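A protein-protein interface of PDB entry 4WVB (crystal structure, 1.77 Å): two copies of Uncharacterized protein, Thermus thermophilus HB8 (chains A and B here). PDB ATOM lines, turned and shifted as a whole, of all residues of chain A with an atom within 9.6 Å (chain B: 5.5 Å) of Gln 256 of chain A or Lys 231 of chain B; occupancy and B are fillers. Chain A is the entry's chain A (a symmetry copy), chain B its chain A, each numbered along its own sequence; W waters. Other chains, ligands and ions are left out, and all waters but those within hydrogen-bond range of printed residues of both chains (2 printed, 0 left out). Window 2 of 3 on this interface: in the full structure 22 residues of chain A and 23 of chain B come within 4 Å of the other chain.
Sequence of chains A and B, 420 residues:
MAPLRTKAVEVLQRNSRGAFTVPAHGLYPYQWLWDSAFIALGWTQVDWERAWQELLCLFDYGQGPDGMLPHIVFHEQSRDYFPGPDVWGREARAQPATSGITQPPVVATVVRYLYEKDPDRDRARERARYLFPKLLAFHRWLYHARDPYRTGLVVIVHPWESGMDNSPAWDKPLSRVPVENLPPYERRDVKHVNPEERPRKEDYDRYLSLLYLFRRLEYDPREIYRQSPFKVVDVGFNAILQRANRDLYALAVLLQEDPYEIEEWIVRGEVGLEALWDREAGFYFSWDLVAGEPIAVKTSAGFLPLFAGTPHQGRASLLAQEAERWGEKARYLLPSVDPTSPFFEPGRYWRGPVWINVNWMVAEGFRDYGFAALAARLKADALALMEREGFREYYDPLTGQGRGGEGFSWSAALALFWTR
NZ of Lys 231 of chain B is in hydrogen-bond range of OE1 of Gln 256 of chain A (2.9 Å). The backbone carbonyl oxygen of Leu 289 of chain B is in hydrogen-bond range of the side-chain amide nitrogen of Gln 256 of chain A (2.9 Å).
The backbone carbonyl oxygen (O) of Tyr 225 of chain B sits at hydrogen-bond distance from the side-chain amino group (NZ) of Lys 231 of chain B (2.7 Å). The backbone carbonyl oxygen (O) of Lys 231 of chain B sits at hydrogen-bond distance from the backbone NH (N) of Leu 289 of chain B. The backbone carbonyl oxygen (O) of Trp 287 of chain B sits at hydrogen-bond distance from the backbone NH (N) of Val 233 of chain B, at 2.8 Å.
CB of Ala 250 of chain A touches CH2 of Trp 287 of chain B, 3.8 Å away. CG1 of Val 253 of chain A touches CZ3 of Trp 287 of chain B (3.7 Å). Leu 289 of chain B touches Val 253 of chain A. Trp 287 of chain B touches Leu 254 of chain A (CE3 to CD2, 3.5 Å). OH of Tyr 225 of chain B touches OE1 of Gln 256 of chain A, at 3.7 Å.
Of the printed residues of chain B, Ala 250 of chain A touches Trp 287. Leu 251 of chain A touches none of the printed residues of chain B. Printed residues of chain B within 4 Å of Val 253 of chain A: Trp 287 (3.7 Å) and Leu 289 (3.7 Å). Of the printed residues of chain B, Leu 254 of chain A touches Trp 287 (3.5 Å). Val 157 of chain B touches none of the printed residues of chain A. Of the printed residues of chain A, Tyr 225 of chain B touches Gln 256. No residue of chain A comes within 4 Å of Phe 230 of chain B. No residue of chain A comes within 4 Å of Val 232 of chain B. Of the printed residues of chain A, Trp 287 of chain B touches Ala 250 (3.8 Å), Val 253 (3.7 Å) and Leu 254 (3.5 Å). Leu 289 of chain B touches just these residues of chain A: Val 253 (3.7 Å) and Gln 256 (2.9 Å). The nearest printed residue of chain A that does not touch Trp 287 of chain B is Tyr 249 of chain A (5.6 Å).
Of the 16 printed residues of chain B, 4 touch a printed residue of chain A. Hydrophobic or aromatic side chains of chain B within 4 Å of the printed part of chain A: Tyr 225, Trp 287 and Leu 289. Among the printed residues, 7 pairs touch across the chains. Among the printed residues, no Asp or Glu carboxylate lies within 4 Å of a Lys or Arg side-chain nitrogen of the other chain.
No position is printed for both chains. Of the 7 pairs that touch across the chains among the printed residues, none has its exchanged pair printed and touching as well.
Water W2 lies within hydrogen-bond range of the backbone carbonyl oxygen (O) of Leu 254 of chain A (2.7 Å) and the backbone carbonyl oxygen (O) of Leu 289 of chain B (2.8 Å). Water W1 bridges the side-chain amino group (NZ) of Lys 231 of chain B (3.0 Å) and the side-chain amide oxygen (OE1) of Gln 256 of chain A (3.3 Å).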
ATOM      1  N   TYR A 115      -7.879  37.812 -16.962  1.00  0.00           N
ATOM      2  CA  TYR A 115      -6.726  37.308 -16.237  1.00  0.00           C
ATOM      3  C   TYR A 115      -5.490  37.113 -17.132  1.00  0.00           C
ATOM      4  O   TYR A 115      -4.391  37.537 -16.769  1.00  0.00           O
ATOM      5  CB  TYR A 115      -7.055  35.980 -15.526  1.00  0.00           C
ATOM      6  CG  TYR A 115      -5.834  35.425 -14.870  1.00  0.00           C
ATOM      7  CD1 TYR A 115      -5.310  36.047 -13.735  1.00  0.00           C
ATOM      8  CD2 TYR A 115      -5.194  34.304 -15.356  1.00  0.00           C
ATOM      9  CE1 TYR A 115      -4.150  35.582 -13.147  1.00  0.00           C
ATOM     10  CE2 TYR A 115      -4.046  33.817 -14.754  1.00  0.00           C
ATOM     11  CZ  TYR A 115      -3.533  34.459 -13.644  1.00  0.00           C
ATOM     12  OH  TYR A 115      -2.396  33.978 -13.046  1.00  0.00           O
ATOM     13  N   ARG A 125      -3.601  38.809 -11.008  1.00  0.00           N
ATOM     14  CA  ARG A 125      -3.633  37.825  -9.931  1.00  0.00           C
ATOM     15  C   ARG A 125      -4.586  38.204  -8.790  1.00  0.00           C
ATOM     16  O   ARG A 125      -5.359  37.372  -8.316  1.00  0.00           O
ATOM     17  CB  ARG A 125      -2.234  37.605  -9.370  1.00  0.00           C
ATOM     18  CG  ARG A 125      -1.359  36.787 -10.294  1.00  0.00           C
ATOM     19  CD  ARG A 125      -0.029  36.400  -9.638  1.00  0.00           C
ATOM     20  NE  ARG A 125       0.979  36.197 -10.674  1.00  0.00           N
ATOM     21  CZ  ARG A 125       1.855  37.113 -11.088  1.00  0.00           C
ATOM     22  NH1 ARG A 125       1.917  38.319 -10.526  1.00  0.00           N
ATOM     23  NH2 ARG A 125       2.696  36.801 -12.062  1.00  0.00           N
ATOM     24  N   ARG A 129      -7.989  35.893  -8.312  1.00  0.00           N
ATOM     25  CA  ARG A 129      -8.046  35.110  -7.067  1.00  0.00           C
ATOM     26  C   ARG A 129      -9.268  35.508  -6.259  1.00  0.00           C
ATOM     27  O   ARG A 129      -9.890  34.672  -5.594  1.00  0.00           O
ATOM     28  CB  ARG A 129      -6.754  35.281  -6.243  1.00  0.00           C
ATOM     29  CG  ARG A 129      -5.535  34.629  -6.907  1.00  0.00           C
ATOM     30  CD  ARG A 129      -4.287  34.561  -6.019  1.00  0.00           C
ATOM     31  NE  ARG A 129      -4.512  33.644  -4.923  1.00  0.00           N
ATOM     32  CZ  ARG A 129      -4.512  32.311  -5.018  1.00  0.00           C
ATOM     33  NH1 ARG A 129      -4.273  31.693  -6.169  1.00  0.00           N
ATOM     34  NH2 ARG A 129      -4.757  31.591  -3.932  1.00  0.00           N
ATOM     35  N   PHE A 132     -12.342  34.047  -8.513  1.00  0.00           N
ATOM     36  CA  PHE A 132     -12.376  32.607  -8.748  1.00  0.00           C
ATOM     37  C   PHE A 132     -13.395  31.853  -7.857  1.00  0.00           C
ATOM     38  O   PHE A 132     -14.240  31.156  -8.377  1.00  0.00           O
ATOM     39  CB  PHE A 132     -10.997  31.936  -8.669  1.00  0.00           C
ATOM     40  CG  PHE A 132     -11.073  30.444  -8.773  1.00  0.00           C
ATOM     41  CD1 PHE A 132     -11.143  29.838 -10.018  1.00  0.00           C
ATOM     42  CD2 PHE A 132     -11.172  29.631  -7.633  1.00  0.00           C
ATOM     43  CE1 PHE A 132     -11.274  28.470 -10.153  1.00  0.00           C
ATOM     44  CE2 PHE A 132     -11.315  28.253  -7.767  1.00  0.00           C
ATOM     45  CZ  PHE A 132     -11.368  27.668  -9.024  1.00  0.00           C
ATOM     46  N   LEU A 248     -13.065  27.987 -16.631  1.00  0.00           N
ATOM     47  CA  LEU A 248     -12.924  28.026 -15.164  1.00  0.00           C
ATOM     48  C   LEU A 248     -11.902  27.003 -14.721  1.00  0.00           C
ATOM     49  O   LEU A 248     -11.109  27.267 -13.803  1.00  0.00           O
ATOM     50  CB  LEU A 248     -14.281  27.819 -14.470  1.00  0.00           C
ATOM     51  CG  LEU A 248     -14.301  28.018 -12.937  1.00  0.00           C
ATOM     52  CD1 LEU A 248     -13.948  29.435 -12.556  1.00  0.00           C
ATOM     53  CD2 LEU A 248     -15.681  27.634 -12.438  1.00  0.00           C
ATOM     54  N   TYR A 249     -11.917  25.835 -15.367  1.00  0.00           N
ATOM     55  CA  TYR A 249     -10.877  24.834 -15.150  1.00  0.00           C
ATOM     56  C   TYR A 249      -9.486  25.410 -15.419  1.00  0.00           C
ATOM     57  O   TYR A 249      -8.576  25.265 -14.604  1.00  0.00           O
ATOM     58  CB  TYR A 249     -11.137  23.576 -16.013  1.00  0.00           C
ATOM     59  CG  TYR A 249      -9.958  22.652 -16.002  1.00  0.00           C
ATOM     60  CD1 TYR A 249      -9.809  21.694 -15.014  1.00  0.00           C
ATOM     61  CD2 TYR A 249      -8.937  22.772 -16.971  1.00  0.00           C
ATOM     62  CE1 TYR A 249      -8.690  20.880 -14.978  1.00  0.00           C
ATOM     63  CE2 TYR A 249      -7.824  21.960 -16.942  1.00  0.00           C
ATOM     64  CZ  TYR A 249      -7.713  20.998 -15.955  1.00  0.00           C
ATOM     65  OH  TYR A 249      -6.592  20.224 -15.929  1.00  0.00           O
ATOM     66  N   ALA A 250      -9.299  26.067 -16.566  1.00  0.00           N
ATOM     67  CA  ALA A 250      -7.998  26.638 -16.921  1.00  0.00           C
ATOM     68  C   ALA A 250      -7.563  27.655 -15.856  1.00  0.00           C
ATOM     69  O   ALA A 250      -6.417  27.639 -15.396  1.00  0.00           O
ATOM     70  CB  ALA A 250      -8.070  27.318 -18.288  1.00  0.00           C
ATOM     71  N   LEU A 251      -8.497  28.494 -15.418  1.00  0.00           N
ATOM     72  CA  LEU A 251      -8.201  29.469 -14.376  1.00  0.00           C
ATOM     73  C   LEU A 251      -7.799  28.765 -13.075  1.00  0.00           C
ATOM     74  O   LEU A 251      -6.842  29.164 -12.418  1.00  0.00           O
ATOM     75  CB  LEU A 251      -9.410  30.348 -14.132  1.00  0.00           C
ATOM     76  CG  LEU A 251      -9.251  31.771 -13.656  1.00  0.00           C
ATOM     77  CD1 LEU A 251      -8.185  32.534 -14.439  1.00  0.00           C
ATOM     78  CD2 LEU A 251     -10.614  32.429 -13.814  1.00  0.00           C
ATOM     79  N   ALA A 252      -8.502  27.700 -12.737  1.00  0.00           N
ATOM     80  CA  ALA A 252      -8.150  26.915 -11.520  1.00  0.00           C
ATOM     81  C   ALA A 252      -6.728  26.364 -11.578  1.00  0.00           C
ATOM     82  O   ALA A 252      -5.974  26.460 -10.606  1.00  0.00           O
ATOM     83  CB  ALA A 252      -9.150  25.774 -11.301  1.00  0.00           C
ATOM     84  N   VAL A 253      -6.336  25.811 -12.726  1.00  0.00           N
ATOM     85  CA  VAL A 253      -4.994  25.263 -12.858  1.00  0.00           C
ATOM     86  C   VAL A 253      -3.935  26.371 -12.798  1.00  0.00           C
ATOM     87  O   VAL A 253      -2.935  26.243 -12.096  1.00  0.00           O
ATOM     88  CB  VAL A 253      -4.867  24.402 -14.145  1.00  0.00           C
ATOM     89  CG1 VAL A 253      -3.410  24.019 -14.412  1.00  0.00           C
ATOM     90  CG2 VAL A 253      -5.792  23.185 -14.043  1.00  0.00           C
ATOM     91  N   LEU A 254      -4.163  27.462 -13.528  1.00  0.00           N
ATOM     92  CA  LEU A 254      -3.224  28.564 -13.536  1.00  0.00           C
ATOM     93  C   LEU A 254      -3.013  29.209 -12.169  1.00  0.00           C
ATOM     94  O   LEU A 254      -1.911  29.633 -11.867  1.00  0.00           O
ATOM     95  CB  LEU A 254      -3.699  29.630 -14.504  1.00  0.00           C
ATOM     96  CG  LEU A 254      -3.513  29.216 -15.977  1.00  0.00           C
ATOM     97  CD1 LEU A 254      -4.329  30.149 -16.878  1.00  0.00           C
ATOM     98  CD2 LEU A 254      -2.049  29.216 -16.379  1.00  0.00           C
ATOM     99  N   LEU A 255      -4.069  29.259 -11.366  1.00  0.00           N
ATOM    100  CA  LEU A 255      -4.028  29.885 -10.031  1.00  0.00           C
ATOM    101  C   LEU A 255      -3.683  28.891  -8.921  1.00  0.00           C
ATOM    102  O   LEU A 255      -3.675  29.255  -7.730  1.00  0.00           O
ATOM    103  CB  LEU A 255      -5.375  30.527  -9.718  1.00  0.00           C
ATOM    104  CG  LEU A 255      -5.825  31.684 -10.613  1.00  0.00           C
ATOM    105  CD1 LEU A 255      -7.220  32.127 -10.242  1.00  0.00           C
ATOM    106  CD2 LEU A 255      -4.832  32.843 -10.521  1.00  0.00           C
ATOM    107  N   GLN A 256      -3.427  27.641  -9.316  1.00  0.00           N
ATOM    108  CA  GLN A 256      -3.261  26.530  -8.380  1.00  0.00           C
ATOM    109  C   GLN A 256      -4.401  26.435  -7.364  1.00  0.00           C
ATOM    110  O   GLN A 256      -4.176  26.245  -6.162  1.00  0.00           O
ATOM    111  CB  GLN A 256      -1.861  26.592  -7.723  1.00  0.00           C
ATOM    112  CG  GLN A 256      -0.724  26.529  -8.728  1.00  0.00           C
ATOM    113  CD  GLN A 256       0.649  26.391  -8.085  1.00  0.00           C
ATOM    114  OE1 GLN A 256       0.933  25.407  -7.395  1.00  0.00           O
ATOM    115  NE2 GLN A 256       1.509  27.377  -8.305  1.00  0.00           N
ATOM    116  N   GLU A 257      -5.631  26.563  -7.865  1.00  0.00           N
ATOM    117  CA  GLU A 257      -6.834  26.302  -7.104  1.00  0.00           C
ATOM    118  C   GLU A 257      -7.228  24.870  -7.364  1.00  0.00           C
ATOM    119  O   GLU A 257      -6.876  24.280  -8.375  1.00  0.00           O
ATOM    120  CB  GLU A 257      -8.006  27.190  -7.540  1.00  0.00           C
ATOM    121  CG  GLU A 257      -7.724  28.674  -7.509  1.00  0.00           C
ATOM    122  CD  GLU A 257      -7.896  29.325  -6.156  1.00  0.00           C
ATOM    123  OE1 GLU A 257      -8.082  28.627  -5.137  1.00  0.00           O
ATOM    124  OE2 GLU A 257      -7.824  30.571  -6.124  1.00  0.00           O
ATOM    125  N   ASP A 258      -8.015  24.334  -6.471  1.00  0.00           N
ATOM    126  CA  ASP A 258      -8.489  22.970  -6.627  1.00  0.00           C
ATOM    127  C   ASP A 258      -9.641  22.833  -7.674  1.00  0.00           C
ATOM    128  O   ASP A 258     -10.663  23.496  -7.585  1.00  0.00           O
ATOM    129  CB  ASP A 258      -8.914  22.449  -5.279  1.00  0.00           C
ATOM    130  CG  ASP A 258      -9.250  20.969  -5.304  1.00  0.00           C
ATOM    131  OD1 ASP A 258      -9.301  20.362  -6.410  1.00  0.00           O
ATOM    132  OD2 ASP A 258      -9.472  20.427  -4.204  1.00  0.00           O
ATOM    133  N   PRO A 259      -9.434  21.979  -8.698  1.00  0.00           N
ATOM    134  CA  PRO A 259     -10.367  21.924  -9.835  1.00  0.00           C
ATOM    135  C   PRO A 259     -11.395  20.807  -9.731  1.00  0.00           C
ATOM    136  O   PRO A 259     -12.152  20.566 -10.679  1.00  0.00           O
ATOM    137  CB  PRO A 259      -9.426  21.669 -11.020  1.00  0.00           C
ATOM    138  CG  PRO A 259      -8.402  20.769 -10.426  1.00  0.00           C
ATOM    139  CD  PRO A 259      -8.177  21.283  -9.024  1.00  0.00           C
ATOM    140  N   TYR A 260     -11.437  20.153  -8.572  1.00  0.00           N
ATOM    141  CA  TYR A 260     -12.273  18.966  -8.321  1.00  0.00           C
ATOM    142  C   TYR A 260     -13.679  19.088  -8.877  1.00  0.00           C
ATOM    143  O   TYR A 260     -14.110  18.251  -9.681  1.00  0.00           O
ATOM    144  CB  TYR A 260     -12.319  18.727  -6.795  1.00  0.00           C
ATOM    145  CG  TYR A 260     -13.056  17.490  -6.354  1.00  0.00           C
ATOM    146  CD1 TYR A 260     -14.441  17.498  -6.187  1.00  0.00           C
ATOM    147  CD2 TYR A 260     -12.360  16.307  -6.073  1.00  0.00           C
ATOM    148  CE1 TYR A 260     -15.125  16.359  -5.790  1.00  0.00           C
ATOM    149  CE2 TYR A 260     -13.034  15.158  -5.657  1.00  0.00           C
ATOM    150  CZ  TYR A 260     -14.414  15.187  -5.524  1.00  0.00           C
ATOM    151  OH  TYR A 260     -15.093  14.051  -5.115  1.00  0.00           O
ATOM    152  N   VAL B 155       3.399  18.632 -13.361  1.00  0.00           N
ATOM    153  CA  VAL B 155       4.452  19.609 -13.482  1.00  0.00           C
ATOM    154  C   VAL B 155       5.854  18.991 -13.573  1.00  0.00           C
ATOM    155  O   VAL B 155       6.150  17.912 -13.043  1.00  0.00           O
ATOM    156  CB  VAL B 155       4.494  20.647 -12.336  1.00  0.00           C
ATOM    157  CG1 VAL B 155       3.198  21.440 -12.229  1.00  0.00           C
ATOM    158  CG2 VAL B 155       4.906  19.984 -11.050  1.00  0.00           C
ATOM    159  N   ILE B 156       6.710  19.701 -14.297  1.00  0.00           N
ATOM    160  CA  ILE B 156       8.130  19.457 -14.224  1.00  0.00           C
ATOM    161  C   ILE B 156       8.683  20.543 -13.297  1.00  0.00           C
ATOM    162  O   ILE B 156       8.234  21.700 -13.341  1.00  0.00           O
ATOM    163  CB  ILE B 156       8.821  19.472 -15.598  1.00  0.00           C
ATOM    164  CG1 ILE B 156       8.533  20.765 -16.381  1.00  0.00           C
ATOM    165  CG2 ILE B 156       8.450  18.215 -16.403  1.00  0.00           C
ATOM    166  CD1 ILE B 156       9.500  20.999 -17.525  1.00  0.00           C
ATOM    167  N   VAL B 157       9.656  20.142 -12.474  1.00  0.00           N
ATOM    168  CA  VAL B 157      10.330  21.029 -11.504  1.00  0.00           C
ATOM    169  C   VAL B 157      11.747  21.385 -11.935  1.00  0.00           C
ATOM    170  O   VAL B 157      12.424  22.183 -11.269  1.00  0.00           O
ATOM    171  CB  VAL B 157      10.279  20.441 -10.059  1.00  0.00           C
ATOM    172  CG1 VAL B 157       8.849  20.357  -9.597  1.00  0.00           C
ATOM    173  CG2 VAL B 157      10.958  19.066  -9.977  1.00  0.00           C
ATOM    174  N   ILE B 224       8.928  19.737  -2.337  1.00  0.00           N
ATOM    175  CA  ILE B 224       9.496  20.271  -3.576  1.00  0.00           C
ATOM    176  C   ILE B 224       8.392  20.827  -4.495  1.00  0.00           C
ATOM    177  O   ILE B 224       8.586  21.841  -5.142  1.00  0.00           O
ATOM    178  CB  ILE B 224      10.352  19.241  -4.320  1.00  0.00           C
ATOM    179  CG1 ILE B 224      11.618  18.945  -3.509  1.00  0.00           C
ATOM    180  CG2 ILE B 224      10.747  19.785  -5.690  1.00  0.00           C
ATOM    181  CD1 ILE B 224      12.335  17.667  -3.873  1.00  0.00           C
ATOM    182  N   TYR B 225       7.247  20.166  -4.545  1.00  0.00           N
ATOM    183  CA  TYR B 225       6.113  20.706  -5.304  1.00  0.00           C
ATOM    184  C   TYR B 225       5.708  22.058  -4.705  1.00  0.00           C
ATOM    185  O   TYR B 225       5.473  23.020  -5.442  1.00  0.00           O
ATOM    186  CB  TYR B 225       4.930  19.724  -5.336  1.00  0.00           C
ATOM    187  CG  TYR B 225       3.769  20.254  -6.145  1.00  0.00           C
ATOM    188  CD1 TYR B 225       2.875  21.145  -5.585  1.00  0.00           C
ATOM    189  CD2 TYR B 225       3.585  19.889  -7.480  1.00  0.00           C
ATOM    190  CE1 TYR B 225       1.840  21.683  -6.317  1.00  0.00           C
ATOM    191  CE2 TYR B 225       2.528  20.420  -8.219  1.00  0.00           C
ATOM    192  CZ  TYR B 225       1.673  21.311  -7.626  1.00  0.00           C
ATOM    193  OH  TYR B 225       0.613  21.859  -8.305  1.00  0.00           O
ATOM    194  N   ARG B 226       5.669  22.145  -3.376  1.00  0.00           N
ATOM    195  CA  ARG B 226       5.330  23.396  -2.709  1.00  0.00           C
ATOM    196  C   ARG B 226       6.365  24.489  -2.961  1.00  0.00           C
ATOM    197  O   ARG B 226       5.994  25.616  -3.257  1.00  0.00           O
ATOM    198  CB  ARG B 226       5.118  23.184  -1.197  1.00  0.00           C
ATOM    199  CG  ARG B 226       3.845  22.404  -0.891  1.00  0.00           C
ATOM    200  CD  ARG B 226       3.671  22.015   0.584  1.00  0.00           C
ATOM    201  NE  ARG B 226       2.417  21.266   0.784  1.00  0.00           N
ATOM    202  CZ  ARG B 226       2.294  20.062   1.364  1.00  0.00           C
ATOM    203  NH1 ARG B 226       3.346  19.420   1.872  1.00  0.00           N
ATOM    204  NH2 ARG B 226       1.089  19.496   1.458  1.00  0.00           N
ATOM    205  N   SER B 228       9.396  24.545  -5.120  1.00  0.00           N
ATOM    206  CA  SER B 228      10.276  24.705  -6.279  1.00  0.00           C
ATOM    207  C   SER B 228      10.048  26.063  -6.937  1.00  0.00           C
ATOM    208  O   SER B 228       8.915  26.416  -7.211  1.00  0.00           O
ATOM    209  CB  SER B 228      10.097  23.599  -7.319  1.00  0.00           C
ATOM    210  OG  SER B 228      11.013  23.821  -8.382  1.00  0.00           O
ATOM    211  N   PRO B 229      11.135  26.824  -7.220  1.00  0.00           N
ATOM    212  CA  PRO B 229      10.953  28.095  -7.928  1.00  0.00           C
ATOM    213  C   PRO B 229      10.719  27.908  -9.431  1.00  0.00           C
ATOM    214  O   PRO B 229      10.475  28.889 -10.125  1.00  0.00           O
ATOM    215  CB  PRO B 229      12.272  28.833  -7.686  1.00  0.00           C
ATOM    216  CG  PRO B 229      13.261  27.783  -7.407  1.00  0.00           C
ATOM    217  CD  PRO B 229      12.523  26.636  -6.767  1.00  0.00           C
ATOM    218  N   PHE B 230      10.850  26.667  -9.904  1.00  0.00           N
ATOM    219  CA  PHE B 230      10.586  26.282 -11.312  1.00  0.00           C
ATOM    220  C   PHE B 230       9.465  25.253 -11.254  1.00  0.00           C
ATOM    221  O   PHE B 230       9.632  24.163 -10.672  1.00  0.00           O
ATOM    222  CB  PHE B 230      11.832  25.667 -11.962  1.00  0.00           C
ATOM    223  CG  PHE B 230      11.689  25.411 -13.444  1.00  0.00           C
ATOM    224  CD1 PHE B 230      11.049  24.272 -13.908  1.00  0.00           C
ATOM    225  CD2 PHE B 230      12.207  26.298 -14.374  1.00  0.00           C
ATOM    226  CE1 PHE B 230      10.937  24.021 -15.252  1.00  0.00           C
ATOM    227  CE2 PHE B 230      12.094  26.065 -15.732  1.00  0.00           C
ATOM    228  CZ  PHE B 230      11.431  24.931 -16.177  1.00  0.00           C
ATOM    229  N   LYS B 231       8.316  25.601 -11.828  1.00  0.00           N
ATOM    230  CA  LYS B 231       7.161  24.729 -11.765  1.00  0.00           C
ATOM    231  C   LYS B 231       6.311  24.964 -12.999  1.00  0.00           C
ATOM    232  O   LYS B 231       5.612  25.969 -13.088  1.00  0.00           O
ATOM    233  CB  LYS B 231       6.366  25.001 -10.509  1.00  0.00           C
ATOM    234  CG  LYS B 231       5.539  23.815 -10.079  1.00  0.00           C
ATOM    235  CD  LYS B 231       5.251  23.855  -8.584  1.00  0.00           C
ATOM    236  CE  LYS B 231       3.947  24.547  -8.260  1.00  0.00           C
ATOM    237  NZ  LYS B 231       3.664  24.493  -6.797  1.00  0.00           N
ATOM    238  N   VAL B 232       6.442  24.055 -13.957  1.00  0.00           N
ATOM    239  CA  VAL B 232       5.894  24.233 -15.292  1.00  0.00           C
ATOM    240  C   VAL B 232       5.074  23.021 -15.719  1.00  0.00           C
ATOM    241  O   VAL B 232       5.494  21.886 -15.574  1.00  0.00           O
ATOM    242  CB  VAL B 232       7.044  24.452 -16.304  1.00  0.00           C
ATOM    243  CG1 VAL B 232       6.542  24.329 -17.743  1.00  0.00           C
ATOM    244  CG2 VAL B 232       7.710  25.804 -16.092  1.00  0.00           C
ATOM    245  N   VAL B 233       3.896  23.285 -16.256  1.00  0.00           N
ATOM    246  CA  VAL B 233       3.152  22.279 -16.999  1.00  0.00           C
ATOM    247  C   VAL B 233       3.661  22.265 -18.450  1.00  0.00           C
ATOM    248  O   VAL B 233       3.309  23.157 -19.243  1.00  0.00           O
ATOM    249  CB  VAL B 233       1.662  22.608 -16.973  1.00  0.00           C
ATOM    250  CG1 VAL B 233       0.872  21.672 -17.853  1.00  0.00           C
ATOM    251  CG2 VAL B 233       1.150  22.574 -15.539  1.00  0.00           C
ATOM    252  N   TRP B 287       2.589  25.895 -19.519  1.00  0.00           N
ATOM    253  CA  TRP B 287       2.149  26.874 -18.546  1.00  0.00           C
ATOM    254  C   TRP B 287       3.147  26.991 -17.400  1.00  0.00           C
ATOM    255  O   TRP B 287       3.704  25.981 -16.934  1.00  0.00           O
ATOM    256  CB  TRP B 287       0.766  26.527 -17.977  1.00  0.00           C
ATOM    257  CG  TRP B 287      -0.373  26.692 -18.925  1.00  0.00           C
ATOM    258  CD1 TRP B 287      -0.325  27.155 -20.219  1.00  0.00           C
ATOM    259  CD2 TRP B 287      -1.742  26.449 -18.644  1.00  0.00           C
ATOM    260  NE1 TRP B 287      -1.576  27.205 -20.747  1.00  0.00           N
ATOM    261  CE2 TRP B 287      -2.470  26.784 -19.797  1.00  0.00           C
ATOM    262  CE3 TRP B 287      -2.435  25.959 -17.523  1.00  0.00           C
ATOM    263  CZ2 TRP B 287      -3.840  26.663 -19.864  1.00  0.00           C
ATOM    264  CZ3 TRP B 287      -3.813  25.829 -17.601  1.00  0.00           C
ATOM    265  CH2 TRP B 287      -4.498  26.187 -18.767  1.00  0.00           C
ATOM    266  N   ASP B 288       3.348  28.221 -16.956  1.00  0.00           N
ATOM    267  CA  ASP B 288       4.240  28.546 -15.842  1.00  0.00           C
ATOM    268  C   ASP B 288       3.374  28.743 -14.598  1.00  0.00           C
ATOM    269  O   ASP B 288       2.634  29.727 -14.490  1.00  0.00           O
ATOM    270  CB  ASP B 288       5.069  29.798 -16.191  1.00  0.00           C
ATOM    271  CG  ASP B 288       5.964  30.293 -15.046  1.00  0.00           C
ATOM    272  OD1 ASP B 288       5.874  29.797 -13.913  1.00  0.00           O
ATOM    273  OD2 ASP B 288       6.789  31.194 -15.308  1.00  0.00           O
ATOM    274  N   LEU B 289       3.428  27.779 -13.678  1.00  0.00           N
ATOM    275  CA  LEU B 289       2.541  27.811 -12.516  1.00  0.00           C
ATOM    276  C   LEU B 289       3.073  28.711 -11.389  1.00  0.00           C
ATOM    277  O   LEU B 289       2.306  29.113 -10.504  1.00  0.00           O
ATOM    278  CB  LEU B 289       2.247  26.395 -12.002  1.00  0.00           C
ATOM    279  CG  LEU B 289       1.527  25.387 -12.906  1.00  0.00           C
ATOM    280  CD1 LEU B 289       0.998  24.231 -12.062  1.00  0.00           C
ATOM    281  CD2 LEU B 289       0.381  26.041 -13.670  1.00  0.00           C
ATOM    282  N   VAL B 290       4.364  29.034 -11.415  1.00  0.00           N
ATOM    283  CA  VAL B 290       4.893  30.051 -10.496  1.00  0.00           C
ATOM    284  C   VAL B 290       4.323  31.424 -10.867  1.00  0.00           C
ATOM    285  O   VAL B 290       3.780  32.119 -10.003  1.00  0.00           O
ATOM    286  CB  VAL B 290       6.440  30.034 -10.422  1.00  0.00           C
ATOM    287  CG1 VAL B 290       6.952  31.155  -9.521  1.00  0.00           C
ATOM    288  CG2 VAL B 290       6.897  28.680  -9.910  1.00  0.00           C
HETATM  289  O   HOH W   1       1.858  24.435  -4.351  1.00  0.00           O
HETATM  290  O   HOH W   2      -0.184  30.226  -9.898  1.00  0.00           O
